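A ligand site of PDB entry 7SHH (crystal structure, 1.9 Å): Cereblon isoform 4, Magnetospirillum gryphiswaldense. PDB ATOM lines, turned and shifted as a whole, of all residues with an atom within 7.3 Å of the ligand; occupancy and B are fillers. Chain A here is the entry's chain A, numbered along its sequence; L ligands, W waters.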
ATOM      1  N   VAL A  49     -24.496  23.408  13.513  1.00  0.00           N
ATOM      2  CA  VAL A  49     -23.043  23.282  13.474  1.00  0.00           C
ATOM      3  C   VAL A  49     -22.401  24.640  13.800  1.00  0.00           C
ATOM      4  O   VAL A  49     -23.033  25.692  13.669  1.00  0.00           O
ATOM      5  CB  VAL A  49     -22.574  22.801  12.087  1.00  0.00           C
ATOM      6  CG1 VAL A  49     -23.006  21.355  11.852  1.00  0.00           C
ATOM      7  CG2 VAL A  49     -23.162  23.695  11.000  1.00  0.00           C
ATOM      8  N   PHE A  50     -21.119  24.582  14.166  1.00  0.00           N
ATOM      9  CA  PHE A  50     -20.297  25.768  14.398  1.00  0.00           C
ATOM     10  C   PHE A  50     -19.071  25.729  13.497  1.00  0.00           C
ATOM     11  O   PHE A  50     -18.467  24.673  13.314  1.00  0.00           O
ATOM     12  CB  PHE A  50     -19.759  25.860  15.826  1.00  0.00           C
ATOM     13  CG  PHE A  50     -20.807  26.006  16.869  1.00  0.00           C
ATOM     14  CD1 PHE A  50     -21.262  24.900  17.558  1.00  0.00           C
ATOM     15  CD2 PHE A  50     -21.302  27.250  17.211  1.00  0.00           C
ATOM     16  CE1 PHE A  50     -22.214  25.038  18.545  1.00  0.00           C
ATOM     17  CE2 PHE A  50     -22.241  27.391  18.193  1.00  0.00           C
ATOM     18  CZ  PHE A  50     -22.705  26.280  18.859  1.00  0.00           C
ATOM     19  N   ASN A  51     -18.695  26.885  12.978  1.00  0.00           N
ATOM     20  CA  ASN A  51     -17.461  26.990  12.217  1.00  0.00           C
ATOM     21  C   ASN A  51     -16.318  27.312  13.169  1.00  0.00           C
ATOM     22  O   ASN A  51     -16.542  27.494  14.375  1.00  0.00           O
ATOM     23  CB  ASN A  51     -17.640  28.018  11.090  1.00  0.00           C
ATOM     24  CG  ASN A  51     -17.743  29.445  11.579  1.00  0.00           C
ATOM     25  OD1 ASN A  51     -17.570  29.744  12.767  1.00  0.00           O
ATOM     26  ND2 ASN A  51     -18.028  30.352  10.646  1.00  0.00           N
ATOM     27  N   PRO A  52     -15.066  27.355  12.702  1.00  0.00           N
ATOM     28  CA  PRO A  52     -13.964  27.647  13.636  1.00  0.00           C
ATOM     29  C   PRO A  52     -14.089  29.003  14.322  1.00  0.00           C
ATOM     30  O   PRO A  52     -13.480  29.203  15.371  1.00  0.00           O
ATOM     31  CB  PRO A  52     -12.716  27.561  12.749  1.00  0.00           C
ATOM     32  CG  PRO A  52     -13.096  26.617  11.668  1.00  0.00           C
ATOM     33  CD  PRO A  52     -14.551  26.889  11.393  1.00  0.00           C
ATOM     34  N   ALA A  53     -14.862  29.928  13.755  1.00  0.00           N
ATOM     35  CA  ALA A  53     -15.076  31.227  14.389  1.00  0.00           C
ATOM     36  C   ALA A  53     -16.190  31.194  15.415  1.00  0.00           C
ATOM     37  O   ALA A  53     -16.579  32.255  15.911  1.00  0.00           O
ATOM     38  CB  ALA A  53     -15.363  32.291  13.335  1.00  0.00           C
ATOM     39  N   PHE A  57     -24.692  27.791  12.886  1.00  0.00           N
ATOM     40  CA  PHE A  57     -25.508  27.738  11.684  1.00  0.00           C
ATOM     41  C   PHE A  57     -26.544  26.637  11.834  1.00  0.00           C
ATOM     42  O   PHE A  57     -26.222  25.531  12.279  1.00  0.00           O
ATOM     43  CB  PHE A  57     -24.664  27.470  10.432  1.00  0.00           C
ATOM     44  CG  PHE A  57     -23.643  28.543  10.138  1.00  0.00           C
ATOM     45  CD1 PHE A  57     -24.001  29.697   9.460  1.00  0.00           C
ATOM     46  CD2 PHE A  57     -22.329  28.390  10.538  1.00  0.00           C
ATOM     47  CE1 PHE A  57     -23.067  30.684   9.217  1.00  0.00           C
ATOM     48  CE2 PHE A  57     -21.387  29.367  10.290  1.00  0.00           C
ATOM     49  CZ  PHE A  57     -21.758  30.518   9.618  1.00  0.00           C
ATOM     50  N   SER A  75     -12.590  22.046  -0.211  1.00  0.00           N
ATOM     51  CA  SER A  75     -11.666  21.856   0.900  1.00  0.00           C
ATOM     52  C   SER A  75     -12.304  20.913   1.912  1.00  0.00           C
ATOM     53  O   SER A  75     -13.511  20.992   2.166  1.00  0.00           O
ATOM     54  CB  SER A  75     -11.315  23.177   1.592  1.00  0.00           C
ATOM     55  OG  SER A  75     -10.667  22.932   2.836  1.00  0.00           O
ATOM     56  N   GLY A  76     -11.507  20.017   2.472  1.00  0.00           N
ATOM     57  CA  GLY A  76     -12.000  19.154   3.515  1.00  0.00           C
ATOM     58  C   GLY A  76     -11.784  19.646   4.930  1.00  0.00           C
ATOM     59  O   GLY A  76     -12.273  19.022   5.868  1.00  0.00           O
ATOM     60  N   GLU A  77     -11.066  20.758   5.102  1.00  0.00           N
ATOM     61  CA  GLU A  77     -10.720  21.234   6.432  1.00  0.00           C
ATOM     62  C   GLU A  77     -11.967  21.651   7.191  1.00  0.00           C
ATOM     63  O   GLU A  77     -12.774  22.438   6.688  1.00  0.00           O
ATOM     64  CB  GLU A  77      -9.726  22.391   6.335  1.00  0.00           C
ATOM     65  CG  GLU A  77      -8.269  21.950   6.200  1.00  0.00           C
ATOM     66  CD  GLU A  77      -7.420  22.929   5.412  1.00  0.00           C
ATOM     67  OE1 GLU A  77      -7.917  24.038   5.090  1.00  0.00           O
ATOM     68  OE2 GLU A  77      -6.256  22.607   5.114  1.00  0.00           O
ATOM     69  N   PHE A  78     -12.132  21.126   8.408  1.00  0.00           N
ATOM     70  CA  PHE A  78     -13.236  21.444   9.298  1.00  0.00           C
ATOM     71  C   PHE A  78     -14.588  21.008   8.747  1.00  0.00           C
ATOM     72  O   PHE A  78     -15.628  21.519   9.186  1.00  0.00           O
ATOM     73  CB  PHE A  78     -13.305  22.953   9.607  1.00  0.00           C
ATOM     74  CG  PHE A  78     -12.037  23.536  10.154  1.00  0.00           C
ATOM     75  CD1 PHE A  78     -11.583  23.193  11.411  1.00  0.00           C
ATOM     76  CD2 PHE A  78     -11.306  24.456   9.410  1.00  0.00           C
ATOM     77  CE1 PHE A  78     -10.418  23.740  11.916  1.00  0.00           C
ATOM     78  CE2 PHE A  78     -10.142  25.003   9.915  1.00  0.00           C
ATOM     79  CZ  PHE A  78      -9.693  24.647  11.173  1.00  0.00           C
ATOM     80  N   SER A  79     -14.621  20.088   7.784  1.00  0.00           N
ATOM     81  CA  SER A  79     -15.891  19.680   7.201  1.00  0.00           C
ATOM     82  C   SER A  79     -16.801  19.065   8.250  1.00  0.00           C
ATOM     83  O   SER A  79     -16.394  18.183   8.999  1.00  0.00           O
ATOM     84  CB  SER A  79     -15.684  18.677   6.067  1.00  0.00           C
ATOM     85  OG  SER A  79     -16.949  18.269   5.570  1.00  0.00           O
ATOM     86  N   TRP A  80     -18.046  19.535   8.308  1.00  0.00           N
ATOM     87  CA  TRP A  80     -19.017  18.996   9.262  1.00  0.00           C
ATOM     88  C   TRP A  80     -19.550  17.631   8.861  1.00  0.00           C
ATOM     89  O   TRP A  80     -20.195  16.968   9.683  1.00  0.00           O
ATOM     90  CB  TRP A  80     -20.211  19.950   9.417  1.00  0.00           C
ATOM     91  CG  TRP A  80     -19.861  21.283   9.965  1.00  0.00           C
ATOM     92  CD1 TRP A  80     -19.129  21.550  11.078  1.00  0.00           C
ATOM     93  CD2 TRP A  80     -20.244  22.548   9.424  1.00  0.00           C
ATOM     94  NE1 TRP A  80     -19.026  22.912  11.268  1.00  0.00           N
ATOM     95  CE2 TRP A  80     -19.710  23.541  10.259  1.00  0.00           C
ATOM     96  CE3 TRP A  80     -21.001  22.937   8.302  1.00  0.00           C
ATOM     97  CZ2 TRP A  80     -19.896  24.902  10.016  1.00  0.00           C
ATOM     98  CZ3 TRP A  80     -21.182  24.281   8.061  1.00  0.00           C
ATOM     99  CH2 TRP A  80     -20.628  25.251   8.915  1.00  0.00           C
ATOM    100  N   PHE A  81     -19.315  17.186   7.635  1.00  0.00           N
ATOM    101  CA  PHE A  81     -19.886  15.948   7.124  1.00  0.00           C
ATOM    102  C   PHE A  81     -18.760  15.015   6.683  1.00  0.00           C
ATOM    103  O   PHE A  81     -18.004  15.351   5.755  1.00  0.00           O
ATOM    104  CB  PHE A  81     -20.850  16.236   5.963  1.00  0.00           C
ATOM    105  CG  PHE A  81     -21.970  17.173   6.324  1.00  0.00           C
ATOM    106  CD1 PHE A  81     -23.083  16.721   6.998  1.00  0.00           C
ATOM    107  CD2 PHE A  81     -21.884  18.516   5.996  1.00  0.00           C
ATOM    108  CE1 PHE A  81     -24.118  17.578   7.322  1.00  0.00           C
ATOM    109  CE2 PHE A  81     -22.915  19.386   6.320  1.00  0.00           C
ATOM    110  CZ  PHE A  81     -24.025  18.910   6.989  1.00  0.00           C
ATOM    111  N   TYR A  84     -16.784  14.440   3.043  1.00  0.00           N
ATOM    112  CA  TYR A  84     -17.184  15.460   2.090  1.00  0.00           C
ATOM    113  C   TYR A  84     -16.249  16.667   2.173  1.00  0.00           C
ATOM    114  O   TYR A  84     -15.807  17.047   3.260  1.00  0.00           O
ATOM    115  CB  TYR A  84     -18.621  15.926   2.340  1.00  0.00           C
ATOM    116  CG  TYR A  84     -19.661  14.864   2.071  1.00  0.00           C
ATOM    117  CD1 TYR A  84     -20.106  14.027   3.090  1.00  0.00           C
ATOM    118  CD2 TYR A  84     -20.202  14.701   0.806  1.00  0.00           C
ATOM    119  CE1 TYR A  84     -21.063  13.054   2.854  1.00  0.00           C
ATOM    120  CE2 TYR A  84     -21.162  13.736   0.548  1.00  0.00           C
ATOM    121  CZ  TYR A  84     -21.583  12.913   1.577  1.00  0.00           C
ATOM    122  OH  TYR A  84     -22.527  11.942   1.336  1.00  0.00           O
ATOM    123  N   ASP A  85     -15.952  17.217   1.003  1.00  0.00           N
ATOM    124  CA  ASP A  85     -15.265  18.486   0.855  1.00  0.00           C
ATOM    125  C   ASP A  85     -16.287  19.559   0.524  1.00  0.00           C
ATOM    126  O   ASP A  85     -17.290  19.287  -0.143  1.00  0.00           O
ATOM    127  CB  ASP A  85     -14.202  18.378  -0.246  1.00  0.00           C
ATOM    128  CG  ASP A  85     -13.281  17.174  -0.050  1.00  0.00           C
ATOM    129  OD1 ASP A  85     -12.873  16.908   1.093  1.00  0.00           O
ATOM    130  OD2 ASP A  85     -13.001  16.480  -1.054  1.00  0.00           O
ATOM    131  N   TRP A  86     -16.048  20.782   0.977  1.00  0.00           N
ATOM    132  CA  TRP A  86     -17.020  21.847   0.821  1.00  0.00           C
ATOM    133  C   TRP A  86     -16.461  22.969  -0.039  1.00  0.00           C
ATOM    134  O   TRP A  86     -15.255  23.231  -0.050  1.00  0.00           O
ATOM    135  CB  TRP A  86     -17.458  22.421   2.176  1.00  0.00           C
ATOM    136  CG  TRP A  86     -16.305  22.790   3.060  1.00  0.00           C
ATOM    137  CD1 TRP A  86     -15.723  22.011   4.015  1.00  0.00           C
ATOM    138  CD2 TRP A  86     -15.602  24.034   3.068  1.00  0.00           C
ATOM    139  NE1 TRP A  86     -14.687  22.694   4.611  1.00  0.00           N
ATOM    140  CE2 TRP A  86     -14.593  23.945   4.054  1.00  0.00           C
ATOM    141  CE3 TRP A  86     -15.729  25.225   2.345  1.00  0.00           C
ATOM    142  CZ2 TRP A  86     -13.717  24.981   4.329  1.00  0.00           C
ATOM    143  CZ3 TRP A  86     -14.850  26.267   2.612  1.00  0.00           C
ATOM    144  CH2 TRP A  86     -13.860  26.133   3.607  1.00  0.00           C
ATOM    145  N   THR A  87     -17.365  23.623  -0.762  1.00  0.00           N
ATOM    146  CA  THR A  87     -17.103  24.897  -1.409  1.00  0.00           C
ATOM    147  C   THR A  87     -18.153  25.899  -0.941  1.00  0.00           C
ATOM    148  O   THR A  87     -19.340  25.549  -0.812  1.00  0.00           O
ATOM    149  CB  THR A  87     -17.148  24.814  -2.939  1.00  0.00           C
ATOM    150  OG1 THR A  87     -18.476  24.479  -3.351  1.00  0.00           O
ATOM    151  CG2 THR A  87     -16.191  23.780  -3.441  1.00  0.00           C
ATOM    152  N   ILE A  88     -17.717  27.132  -0.702  1.00  0.00           N
ATOM    153  CA  ILE A  88     -18.647  28.190  -0.348  1.00  0.00           C
ATOM    154  C   ILE A  88     -19.673  28.367  -1.467  1.00  0.00           C
ATOM    155  O   ILE A  88     -19.322  28.378  -2.655  1.00  0.00           O
ATOM    156  CB  ILE A  88     -17.866  29.485  -0.074  1.00  0.00           C
ATOM    157  CG1 ILE A  88     -17.005  29.315   1.176  1.00  0.00           C
ATOM    158  CG2 ILE A  88     -18.805  30.672   0.073  1.00  0.00           C
ATOM    159  CD1 ILE A  88     -15.818  30.254   1.221  1.00  0.00           C
ATOM    160  N   HIS A  97     -23.932  34.908   1.500  1.00  0.00           N
ATOM    161  CA  HIS A  97     -23.434  33.562   1.792  1.00  0.00           C
ATOM    162  C   HIS A  97     -24.595  32.676   2.228  1.00  0.00           C
ATOM    163  O   HIS A  97     -25.138  32.853   3.319  1.00  0.00           O
ATOM    164  CB  HIS A  97     -22.354  33.614   2.864  1.00  0.00           C
ATOM    165  CG  HIS A  97     -21.833  32.269   3.267  1.00  0.00           C
ATOM    166  ND1 HIS A  97     -21.381  31.988   4.547  1.00  0.00           N
ATOM    167  CD2 HIS A  97     -21.706  31.109   2.565  1.00  0.00           C
ATOM    168  CE1 HIS A  97     -20.987  30.731   4.593  1.00  0.00           C
ATOM    169  NE2 HIS A  97     -21.173  30.179   3.410  1.00  0.00           N
ATOM    170  N   GLY A  99     -24.577  29.107   2.083  1.00  0.00           N
ATOM    171  CA  GLY A  99     -24.207  27.832   2.622  1.00  0.00           C
ATOM    172  C   GLY A  99     -23.002  27.250   1.914  1.00  0.00           C
ATOM    173  O   GLY A  99     -22.074  27.979   1.576  1.00  0.00           O
ATOM    174  N   TRP A 100     -23.022  25.945   1.689  1.00  0.00           N
ATOM    175  CA  TRP A 100     -21.873  25.252   1.110  1.00  0.00           C
ATOM    176  C   TRP A 100     -22.370  24.129   0.213  1.00  0.00           C
ATOM    177  O   TRP A 100     -23.409  23.518   0.466  1.00  0.00           O
ATOM    178  CB  TRP A 100     -20.964  24.657   2.209  1.00  0.00           C
ATOM    179  CG  TRP A 100     -20.498  25.688   3.195  1.00  0.00           C
ATOM    180  CD1 TRP A 100     -19.337  26.407   3.154  1.00  0.00           C
ATOM    181  CD2 TRP A 100     -21.217  26.141   4.344  1.00  0.00           C
ATOM    182  NE1 TRP A 100     -19.290  27.270   4.217  1.00  0.00           N
ATOM    183  CE2 TRP A 100     -20.433  27.137   4.959  1.00  0.00           C
ATOM    184  CE3 TRP A 100     -22.463  25.823   4.906  1.00  0.00           C
ATOM    185  CZ2 TRP A 100     -20.834  27.798   6.126  1.00  0.00           C
ATOM    186  CZ3 TRP A 100     -22.863  26.476   6.052  1.00  0.00           C
ATOM    187  CH2 TRP A 100     -22.051  27.453   6.652  1.00  0.00           C
ATOM    188  N   TYR A 102     -21.241  20.388  -1.019  1.00  0.00           N
ATOM    189  CA  TYR A 102     -20.407  19.285  -0.558  1.00  0.00           C
ATOM    190  C   TYR A 102     -20.227  18.278  -1.681  1.00  0.00           C
ATOM    191  O   TYR A 102     -21.168  18.010  -2.440  1.00  0.00           O
ATOM    192  CB  TYR A 102     -21.023  18.619   0.672  1.00  0.00           C
ATOM    193  CG  TYR A 102     -20.971  19.514   1.891  1.00  0.00           C
ATOM    194  CD1 TYR A 102     -19.880  19.511   2.739  1.00  0.00           C
ATOM    195  CD2 TYR A 102     -22.018  20.404   2.168  1.00  0.00           C
ATOM    196  CE1 TYR A 102     -19.823  20.341   3.850  1.00  0.00           C
ATOM    197  CE2 TYR A 102     -21.977  21.248   3.282  1.00  0.00           C
ATOM    198  CZ  TYR A 102     -20.874  21.210   4.106  1.00  0.00           C
ATOM    199  OH  TYR A 102     -20.807  22.036   5.219  1.00  0.00           O
HETATM  200  C1  LIG L   1     -18.007  23.117   6.872  1.00  0.00           C
HETATM  201  C2  LIG L   1     -16.920  24.609   8.572  1.00  0.00           C
HETATM  202  C3  LIG L   1     -17.056  25.311   6.150  1.00  0.00           C
HETATM  203  C4  LIG L   1     -15.849  26.762   7.765  1.00  0.00           C
HETATM  204  C5  LIG L   1     -16.140  28.236   8.026  1.00  0.00           C
HETATM  205  C6  LIG L   1     -13.711  28.616   8.078  1.00  0.00           C
HETATM  206  C7  LIG L   1     -13.445  27.343   7.846  1.00  0.00           C
HETATM  207  C8  LIG L   1     -14.597  26.349   7.674  1.00  0.00           C
HETATM  208  C9  LIG L   1     -18.149  24.286   5.955  1.00  0.00           C
HETATM  209  C10 LIG L   1     -12.838  30.684   7.447  1.00  0.00           C
HETATM  210  C11 LIG L   1     -17.016  25.812   7.594  1.00  0.00           C
HETATM  211  C12 LIG L   1     -15.155  29.097   8.168  1.00  0.00           C
HETATM  212  N1  LIG L   1     -17.401  23.284   8.147  1.00  0.00           N
HETATM  213  O1  LIG L   1     -18.399  22.040   6.548  1.00  0.00           O
HETATM  214  O2  LIG L   1     -16.497  24.754   9.676  1.00  0.00           O
HETATM  215  O3  LIG L   1     -12.679  29.550   8.235  1.00  0.00           O
HETATM  216  O   HOH W   1     -18.741  30.348   7.581  1.00  0.00           O
HETATM  217  O   HOH W   2     -17.017  29.575   4.967  1.00  0.00           O
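The backbone carbonyl oxygen of Phe 50 is in hydrogen-bond range of the indole nitrogen of Trp 80, 2.8 Å away.
The side-chain amide oxygen (OD1) of Asn 51 sits at hydrogen-bond distance from the backbone NH (N) of Ala 53.
The side-chain hydroxyl of Ser 79 lies within hydrogen-bond range of the backbone carbonyl oxygen of Phe 81 (3.1 Å).
O of Tyr 84 lies within hydrogen-bond range of OG of Ser 79 (2.9 Å).
The backbone carbonyl oxygen (O) of Glu 77 sits at hydrogen-bond distance from the indole nitrogen (NE1) of Trp 86.
O of Ser 75 lies within hydrogen-bond range of N of Trp 86 (2.8 Å).
Merely in contact with the ligand: Asn 51 (3.4 Å), Pro 52 (3.4 Å), Ser 79 (3.5 Å), Trp 86 (3.5 Å) and Trp 100 (3.5 Å).
Hydrophobic or aromatic side chains that line the ligand: Pro 52, Phe 78, Trp 80, Trp 86, Trp 100 and Tyr 102.
Within 4 Å of the ligand: Asn 51, Pro 52, Phe 78, Ser 79, Trp 80, Trp 86, Trp 100 and Tyr 102.
A nitrogen (N1) of the ligand lies within hydrogen-bond range of the backbone carbonyl oxygen (O) of Phe 78, at 2.7 Å.
O1 of the ligand sits at hydrogen-bond distance from OH of Tyr 102 (2.8 Å).
The backbone NH (N) of Trp 80 lies within hydrogen-bond range of an oxygen (O1) of the ligand (3.1 Å).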
